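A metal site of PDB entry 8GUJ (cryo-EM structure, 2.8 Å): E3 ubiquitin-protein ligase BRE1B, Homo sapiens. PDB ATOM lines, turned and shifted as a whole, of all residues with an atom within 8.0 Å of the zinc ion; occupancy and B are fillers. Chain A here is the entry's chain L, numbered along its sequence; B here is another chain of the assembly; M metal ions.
The zinc ion is bound by ND1 of His 965, SG of Cys 986, SG of Cys 983 and SG of Cys 963.
NZ of Lys 985 lies close to ND1 of His 965 (3.5 Å).
O of His 965 is in hydrogen-bond range of N of Leu 960, 3.3 Å away.
The side-chain sulfur of Cys 986 lies close to the backbone NH of Ala 988 (3.8 Å).
SG of Cys 983 lies close to N of Lys 985.
The backbone carbonyl oxygen (O) of Ala 988 is in hydrogen-bond range of the backbone NH (N) of Cys 983 (3.0 Å).
The backbone carbonyl oxygen of Cys 983 lies close to the side-chain amide oxygen of Asn 987 (3.1 Å).
Residues that only touch the zinc ion: Lys 985.
Of the 17 residues printed, 5 come within 4 Å of the zinc ion.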
ATOM      1  N   LEU A 960     -15.322   5.285   1.157  1.00  0.00           N
ATOM      2  CA  LEU A 960     -16.369   4.431   1.692  1.00  0.00           C
ATOM      3  C   LEU A 960     -17.701   5.176   1.561  1.00  0.00           C
ATOM      4  O   LEU A 960     -17.837   6.309   2.018  1.00  0.00           O
ATOM      5  CB  LEU A 960     -16.099   4.085   3.162  1.00  0.00           C
ATOM      6  CG  LEU A 960     -14.653   3.847   3.610  1.00  0.00           C
ATOM      7  CD1 LEU A 960     -14.620   3.497   5.088  1.00  0.00           C
ATOM      8  CD2 LEU A 960     -13.999   2.752   2.797  1.00  0.00           C
ATOM      9  N   LYS A 962     -20.321   4.680   3.139  1.00  0.00           N
ATOM     10  CA  LYS A 962     -21.065   4.736   4.394  1.00  0.00           C
ATOM     11  C   LYS A 962     -20.686   5.918   5.273  1.00  0.00           C
ATOM     12  O   LYS A 962     -21.594   6.605   5.775  1.00  0.00           O
ATOM     13  CB  LYS A 962     -20.852   3.442   5.191  1.00  0.00           C
ATOM     14  CG  LYS A 962     -21.341   2.180   4.493  1.00  0.00           C
ATOM     15  CD  LYS A 962     -22.842   2.249   4.250  1.00  0.00           C
ATOM     16  CE  LYS A 962     -23.602   2.215   5.567  1.00  0.00           C
ATOM     17  NZ  LYS A 962     -23.421   0.934   6.289  1.00  0.00           N
ATOM     18  N   CYS A 963     -19.398   6.179   5.471  1.00  0.00           N
ATOM     19  CA  CYS A 963     -18.959   7.311   6.268  1.00  0.00           C
ATOM     20  C   CYS A 963     -18.600   8.536   5.446  1.00  0.00           C
ATOM     21  O   CYS A 963     -18.319   9.585   6.033  1.00  0.00           O
ATOM     22  CB  CYS A 963     -17.746   6.919   7.131  1.00  0.00           C
ATOM     23  SG  CYS A 963     -16.249   6.603   6.187  1.00  0.00           S
ATOM     24  N   PHE A 964     -18.595   8.419   4.110  1.00  0.00           N
ATOM     25  CA  PHE A 964     -18.354   9.551   3.206  1.00  0.00           C
ATOM     26  C   PHE A 964     -16.976  10.160   3.436  1.00  0.00           C
ATOM     27  O   PHE A 964     -16.805  11.385   3.418  1.00  0.00           O
ATOM     28  CB  PHE A 964     -19.452  10.612   3.344  1.00  0.00           C
ATOM     29  CG  PHE A 964     -20.767  10.242   2.686  1.00  0.00           C
ATOM     30  CD1 PHE A 964     -21.059   8.919   2.363  1.00  0.00           C
ATOM     31  CD2 PHE A 964     -21.713  11.206   2.428  1.00  0.00           C
ATOM     32  CE1 PHE A 964     -22.267   8.596   1.764  1.00  0.00           C
ATOM     33  CE2 PHE A 964     -22.920  10.882   1.829  1.00  0.00           C
ATOM     34  CZ  PHE A 964     -23.194   9.575   1.502  1.00  0.00           C
ATOM     35  N   HIS A 965     -15.982   9.310   3.653  1.00  0.00           N
ATOM     36  CA  HIS A 965     -14.612   9.742   3.878  1.00  0.00           C
ATOM     37  C   HIS A 965     -13.675   9.078   2.879  1.00  0.00           C
ATOM     38  O   HIS A 965     -13.891   7.940   2.461  1.00  0.00           O
ATOM     39  CB  HIS A 965     -14.153   9.432   5.306  1.00  0.00           C
ATOM     40  CG  HIS A 965     -15.061   9.962   6.366  1.00  0.00           C
ATOM     41  ND1 HIS A 965     -15.440   9.216   7.466  1.00  0.00           N
ATOM     42  CD2 HIS A 965     -15.672  11.170   6.505  1.00  0.00           C
ATOM     43  CE1 HIS A 965     -16.241   9.938   8.231  1.00  0.00           C
ATOM     44  NE2 HIS A 965     -16.405  11.120   7.669  1.00  0.00           N
ATOM     45  N   VAL A 966     -12.618   9.799   2.516  1.00  0.00           N
ATOM     46  CA  VAL A 966     -11.698   9.385   1.470  1.00  0.00           C
ATOM     47  C   VAL A 966     -10.497   8.681   2.083  1.00  0.00           C
ATOM     48  O   VAL A 966      -9.889   9.185   3.045  1.00  0.00           O
ATOM     49  CB  VAL A 966     -11.244  10.596   0.620  1.00  0.00           C
ATOM     50  CG1 VAL A 966     -10.487  10.117  -0.612  1.00  0.00           C
ATOM     51  CG2 VAL A 966     -12.427  11.417   0.210  1.00  0.00           C
ATOM     52  N   PHE A 967     -10.185   7.507   1.555  1.00  0.00           N
ATOM     53  CA  PHE A 967      -8.982   6.765   1.933  1.00  0.00           C
ATOM     54  C   PHE A 967      -8.341   6.268   0.636  1.00  0.00           C
ATOM     55  O   PHE A 967      -8.627   6.755  -0.457  1.00  0.00           O
ATOM     56  CB  PHE A 967      -9.285   5.609   2.904  1.00  0.00           C
ATOM     57  CG  PHE A 967      -9.864   6.056   4.234  1.00  0.00           C
ATOM     58  CD1 PHE A 967     -11.171   6.506   4.339  1.00  0.00           C
ATOM     59  CD2 PHE A 967      -9.080   6.017   5.369  1.00  0.00           C
ATOM     60  CE1 PHE A 967     -11.680   6.919   5.550  1.00  0.00           C
ATOM     61  CE2 PHE A 967      -9.590   6.429   6.591  1.00  0.00           C
ATOM     62  CZ  PHE A 967     -10.885   6.878   6.677  1.00  0.00           C
ATOM     63  N   LYS A 982     -14.426  -1.734   9.742  1.00  0.00           N
ATOM     64  CA  LYS A 982     -14.724  -0.465  10.394  1.00  0.00           C
ATOM     65  C   LYS A 982     -13.846   0.598   9.766  1.00  0.00           C
ATOM     66  O   LYS A 982     -12.704   0.336   9.390  1.00  0.00           O
ATOM     67  CB  LYS A 982     -14.479  -0.515  11.907  1.00  0.00           C
ATOM     68  CG  LYS A 982     -15.580  -1.157  12.754  1.00  0.00           C
ATOM     69  CD  LYS A 982     -15.626  -2.673  12.623  1.00  0.00           C
ATOM     70  CE  LYS A 982     -16.659  -3.279  13.551  1.00  0.00           C
ATOM     71  NZ  LYS A 982     -16.795  -4.742  13.343  1.00  0.00           N
ATOM     72  N   CYS A 983     -14.387   1.812   9.640  1.00  0.00           N
ATOM     73  CA  CYS A 983     -13.601   2.906   9.095  1.00  0.00           C
ATOM     74  C   CYS A 983     -12.487   3.260  10.066  1.00  0.00           C
ATOM     75  O   CYS A 983     -12.694   3.243  11.288  1.00  0.00           O
ATOM     76  CB  CYS A 983     -14.487   4.127   8.836  1.00  0.00           C
ATOM     77  SG  CYS A 983     -13.543   5.626   8.534  1.00  0.00           S
ATOM     78  N   PRO A 984     -11.285   3.575   9.566  1.00  0.00           N
ATOM     79  CA  PRO A 984     -10.170   3.875  10.485  1.00  0.00           C
ATOM     80  C   PRO A 984     -10.398   5.076  11.385  1.00  0.00           C
ATOM     81  O   PRO A 984      -9.763   5.152  12.444  1.00  0.00           O
ATOM     82  CB  PRO A 984      -8.996   4.103   9.528  1.00  0.00           C
ATOM     83  CG  PRO A 984      -9.334   3.313   8.319  1.00  0.00           C
ATOM     84  CD  PRO A 984     -10.831   3.385   8.181  1.00  0.00           C
ATOM     85  N   LYS A 985     -11.284   6.007  11.018  1.00  0.00           N
ATOM     86  CA  LYS A 985     -11.468   7.214  11.823  1.00  0.00           C
ATOM     87  C   LYS A 985     -12.835   7.294  12.495  1.00  0.00           C
ATOM     88  O   LYS A 985     -12.903   7.644  13.680  1.00  0.00           O
ATOM     89  CB  LYS A 985     -11.214   8.473  10.977  1.00  0.00           C
ATOM     90  CG  LYS A 985     -12.064   8.609   9.726  1.00  0.00           C
ATOM     91  CD  LYS A 985     -11.791   9.930   9.031  1.00  0.00           C
ATOM     92  CE  LYS A 985     -12.396  11.094   9.804  1.00  0.00           C
ATOM     93  NZ  LYS A 985     -13.850  10.891  10.085  1.00  0.00           N
ATOM     94  N   CYS A 986     -13.925   6.989  11.797  1.00  0.00           N
ATOM     95  CA  CYS A 986     -15.250   7.056  12.402  1.00  0.00           C
ATOM     96  C   CYS A 986     -15.818   5.693  12.767  1.00  0.00           C
ATOM     97  O   CYS A 986     -16.931   5.634  13.303  1.00  0.00           O
ATOM     98  CB  CYS A 986     -16.236   7.783  11.470  1.00  0.00           C
ATOM     99  SG  CYS A 986     -16.589   6.951   9.909  1.00  0.00           S
ATOM    100  N   ASN A 987     -15.091   4.608  12.486  1.00  0.00           N
ATOM    101  CA  ASN A 987     -15.491   3.243  12.819  1.00  0.00           C
ATOM    102  C   ASN A 987     -16.824   2.844  12.214  1.00  0.00           C
ATOM    103  O   ASN A 987     -17.539   2.009  12.771  1.00  0.00           O
ATOM    104  CB  ASN A 987     -15.507   3.027  14.346  1.00  0.00           C
ATOM    105  CG  ASN A 987     -14.212   2.452  14.867  1.00  0.00           C
ATOM    106  OD1 ASN A 987     -13.136   2.759  14.363  1.00  0.00           O
ATOM    107  ND2 ASN A 987     -14.308   1.608  15.883  1.00  0.00           N
ATOM    108  N   ALA A 988     -17.189   3.438  11.076  1.00  0.00           N
ATOM    109  CA  ALA A 988     -18.430   3.081  10.413  1.00  0.00           C
ATOM    110  C   ALA A 988     -18.278   1.754   9.682  1.00  0.00           C
ATOM    111  O   ALA A 988     -17.284   1.526   8.986  1.00  0.00           O
ATOM    112  CB  ALA A 988     -18.864   4.173   9.444  1.00  0.00           C
ATOM    113  N   ALA A 989     -19.270   0.880   9.830  1.00  0.00           N
ATOM    114  CA  ALA A 989     -19.239  -0.409   9.168  1.00  0.00           C
ATOM    115  C   ALA A 989     -19.502  -0.256   7.682  1.00  0.00           C
ATOM    116  O   ALA A 989     -20.420   0.443   7.264  1.00  0.00           O
ATOM    117  CB  ALA A 989     -20.270  -1.353   9.792  1.00  0.00           C
ATOM    118  N   PHE A 990     -18.671  -0.923   6.871  1.00  0.00           N
ATOM    119  CA  PHE A 990     -18.795  -0.868   5.422  1.00  0.00           C
ATOM    120  C   PHE A 990     -18.709  -2.279   4.859  1.00  0.00           C
ATOM    121  O   PHE A 990     -18.079  -3.172   5.437  1.00  0.00           O
ATOM    122  CB  PHE A 990     -17.733   0.050   4.798  1.00  0.00           C
ATOM    123  CG  PHE A 990     -16.315  -0.387   5.068  1.00  0.00           C
ATOM    124  CD1 PHE A 990     -15.683  -0.047   6.250  1.00  0.00           C
ATOM    125  CD2 PHE A 990     -15.619  -1.124   4.125  1.00  0.00           C
ATOM    126  CE1 PHE A 990     -14.388  -0.442   6.496  1.00  0.00           C
ATOM    127  CE2 PHE A 990     -14.313  -1.521   4.362  1.00  0.00           C
ATOM    128  CZ  PHE A 990     -13.701  -1.174   5.553  1.00  0.00           C
ATOM    129  N   TYR B 973     -16.013  14.192   1.919  1.00  0.00           N
ATOM    130  CA  TYR B 973     -14.915  14.877   2.632  1.00  0.00           C
ATOM    131  C   TYR B 973     -13.562  14.445   2.063  1.00  0.00           C
ATOM    132  O   TYR B 973     -12.926  13.530   2.585  1.00  0.00           O
ATOM    133  CB  TYR B 973     -14.956  14.609   4.144  1.00  0.00           C
ATOM    134  CG  TYR B 973     -16.106  15.236   4.901  1.00  0.00           C
ATOM    135  CD1 TYR B 973     -16.871  16.244   4.343  1.00  0.00           C
ATOM    136  CD2 TYR B 973     -16.412  14.802   6.189  1.00  0.00           C
ATOM    137  CE1 TYR B 973     -17.918  16.822   5.057  1.00  0.00           C
ATOM    138  CE2 TYR B 973     -17.454  15.367   6.901  1.00  0.00           C
ATOM    139  CZ  TYR B 973     -18.207  16.375   6.324  1.00  0.00           C
ATOM    140  OH  TYR B 973     -19.249  16.940   7.037  1.00  0.00           O
HETATM  141 ZN    ZN M   1     -15.141   7.259   8.126  1.00  0.00          ZN
